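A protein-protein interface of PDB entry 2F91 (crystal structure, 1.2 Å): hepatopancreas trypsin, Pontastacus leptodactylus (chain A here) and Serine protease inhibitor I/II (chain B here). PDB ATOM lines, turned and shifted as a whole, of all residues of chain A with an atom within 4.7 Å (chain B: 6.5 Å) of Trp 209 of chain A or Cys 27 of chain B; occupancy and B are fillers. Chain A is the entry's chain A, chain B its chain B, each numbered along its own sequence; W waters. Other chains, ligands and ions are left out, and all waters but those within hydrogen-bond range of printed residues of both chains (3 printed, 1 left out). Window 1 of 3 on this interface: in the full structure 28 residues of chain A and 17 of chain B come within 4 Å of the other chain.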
ATOM      1  N   LEU A  92     -18.665 -16.646  31.095  1.00  0.00           N
ATOM      2  CA  LEU A  92     -18.916 -17.974  31.652  1.00  0.00           C
ATOM      3  C   LEU A  92     -20.262 -18.561  31.292  1.00  0.00           C
ATOM      4  O   LEU A  92     -20.517 -19.765  31.478  1.00  0.00           O
ATOM      5  CB  LEU A  92     -18.750 -17.897  33.171  1.00  0.00           C
ATOM      6  CG  LEU A  92     -17.317 -17.594  33.620  1.00  0.00           C
ATOM      7  CD1 LEU A  92     -17.285 -17.290  35.116  1.00  0.00           C
ATOM      8  CD2 LEU A  92     -16.381 -18.755  33.278  1.00  0.00           C
ATOM      9  N   LEU A  93     -21.141 -17.789  30.698  1.00  0.00           N
ATOM     10  CA  LEU A  93     -22.403 -18.227  30.116  1.00  0.00           C
ATOM     11  C   LEU A  93     -23.385 -18.673  31.186  1.00  0.00           C
ATOM     12  O   LEU A  93     -24.262 -19.485  30.975  1.00  0.00           O
ATOM     13  CB  LEU A  93     -22.243 -19.259  28.996  1.00  0.00           C
ATOM     14  CG  LEU A  93     -21.303 -18.780  27.878  1.00  0.00           C
ATOM     15  CD1 LEU A  93     -21.092 -19.894  26.895  1.00  0.00           C
ATOM     16  CD2 LEU A  93     -21.840 -17.510  27.201  1.00  0.00           C
ATOM     17  N   TYR A 163     -15.256 -30.652  32.731  1.00  0.00           N
ATOM     18  CA  TYR A 163     -15.162 -29.208  32.504  1.00  0.00           C
ATOM     19  C   TYR A 163     -14.761 -28.400  33.714  1.00  0.00           C
ATOM     20  O   TYR A 163     -14.323 -27.250  33.580  1.00  0.00           O
ATOM     21  CB  TYR A 163     -16.491 -28.728  31.956  1.00  0.00           C
ATOM     22  CG  TYR A 163     -16.833 -29.085  30.538  1.00  0.00           C
ATOM     23  CD1 TYR A 163     -16.030 -28.650  29.487  1.00  0.00           C
ATOM     24  CD2 TYR A 163     -17.957 -29.813  30.236  1.00  0.00           C
ATOM     25  CE1 TYR A 163     -16.353 -28.951  28.180  1.00  0.00           C
ATOM     26  CE2 TYR A 163     -18.282 -30.106  28.943  1.00  0.00           C
ATOM     27  CZ  TYR A 163     -17.457 -29.697  27.920  1.00  0.00           C
ATOM     28  OH  TYR A 163     -17.788 -29.986  26.608  1.00  0.00           O
ATOM     29  N   GLU A 167     -17.453 -24.563  36.584  1.00  0.00           N
ATOM     30  CA  GLU A 167     -17.752 -24.266  35.177  1.00  0.00           C
ATOM     31  C   GLU A 167     -19.133 -24.750  34.758  1.00  0.00           C
ATOM     32  O   GLU A 167     -19.769 -24.166  33.900  1.00  0.00           O
ATOM     33  CB  GLU A 167     -16.694 -24.928  34.282  1.00  0.00           C
ATOM     34  CG  GLU A 167     -16.723 -24.416  32.837  1.00  0.00           C
ATOM     35  CD  GLU A 167     -16.052 -23.090  32.563  1.00  0.00           C
ATOM     36  OE1 GLU A 167     -15.413 -22.480  33.421  1.00  0.00           O
ATOM     37  OE2 GLU A 167     -16.136 -22.658  31.357  1.00  0.00           O
ATOM     38  N   ILE A 168     -19.546 -25.858  35.352  1.00  0.00           N
ATOM     39  CA  ILE A 168     -20.888 -26.390  35.151  1.00  0.00           C
ATOM     40  C   ILE A 168     -21.737 -25.957  36.325  1.00  0.00           C
ATOM     41  O   ILE A 168     -21.553 -26.445  37.438  1.00  0.00           O
ATOM     42  CB  ILE A 168     -20.892 -27.911  35.000  1.00  0.00           C
ATOM     43  CG1 ILE A 168     -19.942 -28.377  33.889  1.00  0.00           C
ATOM     44  CG2 ILE A 168     -22.311 -28.405  34.814  1.00  0.00           C
ATOM     45  CD1 ILE A 168     -20.364 -27.873  32.532  1.00  0.00           C
ATOM     46  N   MET A 172     -27.189 -25.375  34.360  1.00  0.00           N
ATOM     47  CA  MET A 172     -26.761 -25.919  33.069  1.00  0.00           C
ATOM     48  C   MET A 172     -27.135 -27.414  33.049  1.00  0.00           C
ATOM     49  O   MET A 172     -27.193 -28.052  34.103  1.00  0.00           O
ATOM     50  CB  MET A 172     -25.279 -25.752  32.807  1.00  0.00           C
ATOM     51  CG  MET A 172     -24.886 -24.266  32.631  1.00  0.00           C
ATOM     52  SD  MET A 172     -23.102 -24.103  32.775  1.00  0.00           S
ATOM     53  CE  MET A 172     -22.957 -22.292  32.820  1.00  0.00           C
ATOM     54  N   GLN A 186     -21.469 -25.710  16.130  1.00  0.00           N
ATOM     55  CA  GLN A 186     -21.564 -24.327  15.708  1.00  0.00           C
ATOM     56  C   GLN A 186     -22.724 -24.119  14.727  1.00  0.00           C
ATOM     57  O   GLN A 186     -22.815 -24.779  13.703  1.00  0.00           O
ATOM     58  CB  GLN A 186     -20.234 -23.870  15.122  1.00  0.00           C
ATOM     59  CG  GLN A 186     -19.252 -23.387  16.163  1.00  0.00           C
ATOM     60  CD  GLN A 186     -18.730 -24.411  17.146  1.00  0.00           C
ATOM     61  OE1 GLN A 186     -18.401 -25.522  16.680  1.00  0.00           O
ATOM     62  NE2 GLN A 186     -18.605 -24.139  18.459  1.00  0.00           N
ATOM     63  N   VAL A 207     -29.242 -24.865  23.486  1.00  0.00           N
ATOM     64  CA  VAL A 207     -27.825 -25.083  23.142  1.00  0.00           C
ATOM     65  C   VAL A 207     -26.964 -23.904  23.534  1.00  0.00           C
ATOM     66  O   VAL A 207     -27.283 -22.760  23.199  1.00  0.00           O
ATOM     67  CB  VAL A 207     -27.668 -25.302  21.624  1.00  0.00           C
ATOM     68  CG1 VAL A 207     -26.221 -25.485  21.190  1.00  0.00           C
ATOM     69  CG2 VAL A 207     -28.497 -26.494  21.130  1.00  0.00           C
ATOM     70  N   SER A 208     -25.879 -24.160  24.251  1.00  0.00           N
ATOM     71  CA  SER A 208     -25.031 -23.086  24.802  1.00  0.00           C
ATOM     72  C   SER A 208     -23.567 -23.225  24.406  1.00  0.00           C
ATOM     73  O   SER A 208     -23.023 -22.368  23.676  1.00  0.00           O
ATOM     74  CB  SER A 208     -25.208 -23.031  26.312  1.00  0.00           C
ATOM     75  OG  SER A 208     -24.553 -21.904  26.894  1.00  0.00           O
ATOM     76  N   TRP A 209     -22.843 -24.221  24.838  1.00  0.00           N
ATOM     77  CA  TRP A 209     -21.379 -24.272  24.652  1.00  0.00           C
ATOM     78  C   TRP A 209     -20.873 -25.692  24.753  1.00  0.00           C
ATOM     79  O   TRP A 209     -21.577 -26.630  25.138  1.00  0.00           O
ATOM     80  CB  TRP A 209     -20.699 -23.365  25.630  1.00  0.00           C
ATOM     81  CG  TRP A 209     -20.841 -23.649  27.086  1.00  0.00           C
ATOM     82  CD1 TRP A 209     -21.855 -23.148  27.896  1.00  0.00           C
ATOM     83  CD2 TRP A 209     -19.985 -24.416  27.934  1.00  0.00           C
ATOM     84  NE1 TRP A 209     -21.646 -23.606  29.190  1.00  0.00           N
ATOM     85  CE2 TRP A 209     -20.530 -24.366  29.240  1.00  0.00           C
ATOM     86  CE3 TRP A 209     -18.816 -25.154  27.745  1.00  0.00           C
ATOM     87  CZ2 TRP A 209     -19.943 -25.015  30.326  1.00  0.00           C
ATOM     88  CZ3 TRP A 209     -18.230 -25.803  28.801  1.00  0.00           C
ATOM     89  CH2 TRP A 209     -18.786 -25.739  30.075  1.00  0.00           C
ATOM     90  N   GLY A 210     -19.596 -25.867  24.425  1.00  0.00           N
ATOM     91  CA  GLY A 210     -18.867 -27.093  24.654  1.00  0.00           C
ATOM     92  C   GLY A 210     -17.408 -26.938  24.289  1.00  0.00           C
ATOM     93  O   GLY A 210     -17.030 -25.897  23.714  1.00  0.00           O
ATOM     94  N   GLY A 220     -22.010 -31.798  25.271  1.00  0.00           N
ATOM     95  CA  GLY A 220     -22.529 -30.461  25.071  1.00  0.00           C
ATOM     96  C   GLY A 220     -23.141 -29.930  26.343  1.00  0.00           C
ATOM     97  O   GLY A 220     -23.680 -30.673  27.167  1.00  0.00           O
ATOM     98  N   VAL A 221     -23.096 -28.606  26.483  1.00  0.00           N
ATOM     99  CA  VAL A 221     -23.652 -27.908  27.634  1.00  0.00           C
ATOM    100  C   VAL A 221     -24.753 -26.961  27.172  1.00  0.00           C
ATOM    101  O   VAL A 221     -24.636 -26.256  26.176  1.00  0.00           O
ATOM    102  CB  VAL A 221     -22.570 -27.162  28.435  1.00  0.00           C
ATOM    103  CG1 VAL A 221     -23.112 -26.640  29.751  1.00  0.00           C
ATOM    104  CG2 VAL A 221     -21.413 -28.081  28.687  1.00  0.00           C
ATOM    105  N   LYS B  10     -10.719 -16.060  24.806  1.00  0.00           N
ATOM    106  CA  LYS B  10     -10.341 -15.807  23.427  1.00  0.00           C
ATOM    107  C   LYS B  10     -11.593 -15.810  22.577  1.00  0.00           C
ATOM    108  O   LYS B  10     -12.693 -16.147  23.017  1.00  0.00           O
ATOM    109  CB  LYS B  10      -9.315 -16.817  22.895  1.00  0.00           C
ATOM    110  CG  LYS B  10      -9.857 -18.194  22.637  1.00  0.00           C
ATOM    111  CD  LYS B  10      -8.925 -19.060  21.823  1.00  0.00           C
ATOM    112  CE  LYS B  10      -9.499 -20.442  21.560  1.00  0.00           C
ATOM    113  NZ  LYS B  10      -8.745 -21.143  20.466  1.00  0.00           N
ATOM    114  N   LYS B  11     -11.454 -15.458  21.307  1.00  0.00           N
ATOM    115  CA  LYS B  11     -12.501 -15.702  20.323  1.00  0.00           C
ATOM    116  C   LYS B  11     -11.999 -16.824  19.403  1.00  0.00           C
ATOM    117  O   LYS B  11     -10.800 -17.024  19.210  1.00  0.00           O
ATOM    118  CB  LYS B  11     -12.846 -14.482  19.493  1.00  0.00           C
ATOM    119  CG  LYS B  11     -13.350 -13.283  20.283  1.00  0.00           C
ATOM    120  CD  LYS B  11     -14.494 -12.583  19.569  1.00  0.00           C
ATOM    121  N   GLN B  12     -12.933 -17.558  18.856  1.00  0.00           N
ATOM    122  CA  GLN B  12     -12.740 -18.585  17.841  1.00  0.00           C
ATOM    123  C   GLN B  12     -13.704 -18.195  16.756  1.00  0.00           C
ATOM    124  O   GLN B  12     -14.904 -18.434  16.831  1.00  0.00           O
ATOM    125  CB  GLN B  12     -12.974 -19.977  18.404  1.00  0.00           C
ATOM    126  CG  GLN B  12     -12.930 -21.052  17.340  1.00  0.00           C
ATOM    127  CD  GLN B  12     -13.726 -22.303  17.686  1.00  0.00           C
ATOM    128  OE1 GLN B  12     -14.861 -22.492  17.212  1.00  0.00           O
ATOM    129  NE2 GLN B  12     -13.095 -23.145  18.507  1.00  0.00           N
ATOM    130  N   ASN B  15     -17.247 -16.896  17.678  1.00  0.00           N
ATOM    131  CA  ASN B  15     -17.608 -17.467  18.980  1.00  0.00           C
ATOM    132  C   ASN B  15     -16.628 -17.013  20.047  1.00  0.00           C
ATOM    133  O   ASN B  15     -15.457 -16.641  19.798  1.00  0.00           O
ATOM    134  CB  ASN B  15     -17.704 -19.002  18.866  1.00  0.00           C
ATOM    135  CG  ASN B  15     -19.012 -19.383  18.245  1.00  0.00           C
ATOM    136  OD1 ASN B  15     -20.073 -19.069  18.783  1.00  0.00           O
ATOM    137  ND2 ASN B  15     -18.947 -20.019  17.079  1.00  0.00           N
ATOM    138  N   THR B  16     -17.120 -17.048  21.288  1.00  0.00           N
ATOM    139  CA  THR B  16     -16.392 -16.620  22.459  1.00  0.00           C
ATOM    140  C   THR B  16     -16.081 -17.839  23.297  1.00  0.00           C
ATOM    141  O   THR B  16     -16.892 -18.753  23.352  1.00  0.00           O
ATOM    142  CB  THR B  16     -17.163 -15.610  23.306  1.00  0.00           C
ATOM    143  OG1 THR B  16     -18.466 -16.124  23.608  1.00  0.00           O
ATOM    144  CG2 THR B  16     -17.388 -14.327  22.550  1.00  0.00           C
ATOM    145  N   CYS B  17     -14.914 -17.831  23.892  1.00  0.00           N
ATOM    146  CA  CYS B  17     -14.382 -18.934  24.648  1.00  0.00           C
ATOM    147  C   CYS B  17     -13.741 -18.514  25.973  1.00  0.00           C
ATOM    148  O   CYS B  17     -13.155 -17.436  26.079  1.00  0.00           O
ATOM    149  CB  CYS B  17     -13.295 -19.689  23.842  1.00  0.00           C
ATOM    150  SG  CYS B  17     -13.674 -20.023  22.097  1.00  0.00           S
ATOM    151  N   ASN B  18     -13.871 -19.411  26.939  1.00  0.00           N
ATOM    152  CA  ASN B  18     -13.133 -19.280  28.193  1.00  0.00           C
ATOM    153  C   ASN B  18     -12.415 -20.588  28.502  1.00  0.00           C
ATOM    154  O   ASN B  18     -12.924 -21.649  28.145  1.00  0.00           O
ATOM    155  CB  ASN B  18     -14.022 -18.807  29.346  1.00  0.00           C
ATOM    156  CG  ASN B  18     -15.053 -19.824  29.770  1.00  0.00           C
ATOM    157  OD1 ASN B  18     -16.193 -19.897  29.301  1.00  0.00           O
ATOM    158  ND2 ASN B  18     -14.630 -20.633  30.705  1.00  0.00           N
ATOM    159  N   THR B  20     -11.515 -23.437  30.810  1.00  0.00           N
ATOM    160  CA  THR B  20     -12.126 -24.027  31.994  1.00  0.00           C
ATOM    161  C   THR B  20     -11.101 -24.379  33.049  1.00  0.00           C
ATOM    162  O   THR B  20      -9.881 -24.394  32.795  1.00  0.00           O
ATOM    163  CB  THR B  20     -12.851 -25.368  31.669  1.00  0.00           C
ATOM    164  OG1 THR B  20     -11.800 -26.283  31.315  1.00  0.00           O
ATOM    165  CG2 THR B  20     -13.771 -25.209  30.485  1.00  0.00           C
ATOM    166  N   TRP B  25     -10.956 -25.332  26.156  1.00  0.00           N
ATOM    167  CA  TRP B  25     -11.684 -24.159  25.691  1.00  0.00           C
ATOM    168  C   TRP B  25     -13.175 -24.436  25.614  1.00  0.00           C
ATOM    169  O   TRP B  25     -13.586 -25.233  24.771  1.00  0.00           O
ATOM    170  CB  TRP B  25     -11.200 -23.681  24.332  1.00  0.00           C
ATOM    171  CG  TRP B  25      -9.866 -23.015  24.372  1.00  0.00           C
ATOM    172  CD1 TRP B  25      -8.711 -23.521  23.856  1.00  0.00           C
ATOM    173  CD2 TRP B  25      -9.560 -21.753  24.964  1.00  0.00           C
ATOM    174  NE1 TRP B  25      -7.720 -22.624  24.106  1.00  0.00           N
ATOM    175  CE2 TRP B  25      -8.187 -21.536  24.774  1.00  0.00           C
ATOM    176  CE3 TRP B  25     -10.341 -20.791  25.637  1.00  0.00           C
ATOM    177  CZ2 TRP B  25      -7.580 -20.384  25.237  1.00  0.00           C
ATOM    178  CZ3 TRP B  25      -9.698 -19.631  26.100  1.00  0.00           C
ATOM    179  CH2 TRP B  25      -8.320 -19.450  25.889  1.00  0.00           C
ATOM    180  N   ALA B  26     -13.933 -23.765  26.460  1.00  0.00           N
ATOM    181  CA  ALA B  26     -15.370 -23.782  26.459  1.00  0.00           C
ATOM    182  C   ALA B  26     -15.819 -22.710  25.459  1.00  0.00           C
ATOM    183  O   ALA B  26     -15.616 -21.528  25.770  1.00  0.00           O
ATOM    184  CB  ALA B  26     -15.920 -23.478  27.844  1.00  0.00           C
ATOM    185  N   CYS B  27     -16.385 -23.082  24.326  1.00  0.00           N
ATOM    186  CA  CYS B  27     -16.736 -22.144  23.262  1.00  0.00           C
ATOM    187  C   CYS B  27     -18.215 -22.153  22.923  1.00  0.00           C
ATOM    188  O   CYS B  27     -18.821 -23.229  22.900  1.00  0.00           O
ATOM    189  CB  CYS B  27     -15.969 -22.434  21.968  1.00  0.00           C
ATOM    190  SG  CYS B  27     -14.196 -22.105  22.128  1.00  0.00           S
ATOM    191  N   THR B  28     -18.757 -20.983  22.663  1.00  0.00           N
ATOM    192  CA  THR B  28     -20.136 -20.912  22.169  1.00  0.00           C
ATOM    193  C   THR B  28     -20.283 -21.575  20.767  1.00  0.00           C
ATOM    194  O   THR B  28     -19.342 -21.820  20.098  1.00  0.00           O
ATOM    195  CB  THR B  28     -20.561 -19.500  22.178  1.00  0.00           C
ATOM    196  OG1 THR B  28     -19.691 -18.708  21.320  1.00  0.00           O
ATOM    197  CG2 THR B  28     -20.705 -18.788  23.533  1.00  0.00           C
ATOM    198  N   ARG B  29     -21.574 -21.770  20.472  1.00  0.00           N
ATOM    199  CA  ARG B  29     -21.972 -22.565  19.337  1.00  0.00           C
ATOM    200  C   ARG B  29     -22.789 -21.793  18.288  1.00  0.00           C
ATOM    201  O   ARG B  29     -23.701 -22.307  17.624  1.00  0.00           O
ATOM    202  CB  ARG B  29     -22.557 -23.926  19.851  1.00  0.00           C
ATOM    203  CG  ARG B  29     -21.586 -24.825  20.408  1.00  0.00           C
ATOM    204  CD  ARG B  29     -22.289 -26.037  21.024  1.00  0.00           C
ATOM    205  NE  ARG B  29     -21.186 -26.942  21.380  1.00  0.00           N
ATOM    206  CZ  ARG B  29     -21.349 -28.190  21.749  1.00  0.00           C
ATOM    207  NH1 ARG B  29     -22.546 -28.659  21.993  1.00  0.00           N
ATOM    208  NH2 ARG B  29     -20.331 -29.015  21.919  1.00  0.00           N
HETATM  209  O   HOH W   1     -24.703 -27.329  23.627  1.00  0.00           O
HETATM  210  O   HOH W   2     -18.362 -25.897  21.060  1.00  0.00           O
HETATM  211  O   HOH W   3     -18.755 -21.339  29.388  1.00  0.00           O
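Leu 92 of chain A touches Asn 18 of chain B.
Glu 167 of chain A touches Thr 20 of chain B.
OE2 of Glu 167 of chain A touches CB of Ala 26 of chain B, 3.6 Å away.
ND2 of Asn 15 of chain B touches CG of Gln 186 of chain A (3.5 Å).
Arg 29 of chain B touches Gln 186 of chain A.
Ala 26 of chain B touches Trp 209 of chain A.
Cys 27 of chain B touches Trp 209 of chain A.
Gly 210 of chain A touches Trp 25 of chain B.
Gly 210 of chain A touches Ala 26 of chain B (O to C, 3.8 Å).
Arg 29 of chain B touches Gly 210 of chain A (NE to N, 3.6 Å).
The backbone NH (N) of Cys 27 of chain B is in hydrogen-bond range of the backbone carbonyl oxygen (O) of Gly 210 of chain A, at 3.0 Å.
O of Thr 28 of chain B sits at hydrogen-bond distance from NE2 of Gln 186 of chain A (2.9 Å).
The side-chain amide nitrogen of Asn 18 of chain B is in hydrogen-bond range of the side-chain carboxylate of Glu 167 of chain A (2.6 Å).
The backbone carbonyl oxygen of Val 221 of chain A sits at hydrogen-bond distance from the backbone NH of Ser 208 of chain A (3.1 Å).
The backbone carbonyl oxygen (O) of Asn 18 of chain B sits at hydrogen-bond distance from the backbone NH (N) of Ala 26 of chain B.
The side-chain sulfur (SG) of Cys 17 of chain B is disulfide-bonded to the side-chain sulfur (SG) of Cys 27 of chain B, 2.1 Å away.
The side-chain amide oxygen (OD1) of Asn 15 of chain B lies within hydrogen-bond range of the side-chain hydroxyl (OG1) of Thr 28 of chain B (2.6 Å).
N of Val 221 of chain A lies within hydrogen-bond range of O of Trp 209 of chain A, at 2.8 Å.
The backbone carbonyl oxygen (O) of Thr 16 of chain B lies within hydrogen-bond range of the backbone NH (N) of Thr 28 of chain B, at 3.0 Å.
Of the 13 printed residues of chain A, 10 touch a printed residue of chain B.
Hydrophobic or aromatic side chains of chain A within 4 Å of the printed part of chain B: Leu 92, Leu 93, Val 207 and Trp 209.
Hydrophobic or aromatic side chains of chain B that line the printed part of chain A: Ala 26.
Among the printed residues, 20 pairs touch across the chains.
Water W1 lies within hydrogen-bond range of O of Val 221 of chain A (2.8 Å), NH1 of Arg 29 of chain B (3.0 Å) and N of Ser 208 of chain A (3.4 Å).
Water W3 bridges the side-chain amide oxygen (OD1) of Asn 18 of chain B and the backbone carbonyl oxygen (O) of Leu 92 of chain A.
Water W2 lies within hydrogen-bond range of O of Gly 210 of chain A, NE of Arg 29 of chain B, NE2 of Gln 186 of chain A and O of Cys 27 of chain B.
Of the printed residues of chain B, Trp 209 of chain A touches Ala 26, Cys 27 and Arg 29.
Of the printed residues of chain A, Cys 27 of chain B touches Trp 209 and Gly 210.
Of the printed residues of chain B, Ser 208 of chain A touches Thr 28 and Arg 29.
Of the printed residues of chain B, Glu 167 of chain A touches Asn 18, Thr 20 and Ala 26.
Of the printed residues of chain A, Arg 29 of chain B touches Gln 186, Val 207, Ser 208, Trp 209, Gly 210 and Gly 220.
Met 172 of chain A touches none of the printed residues of chain B.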
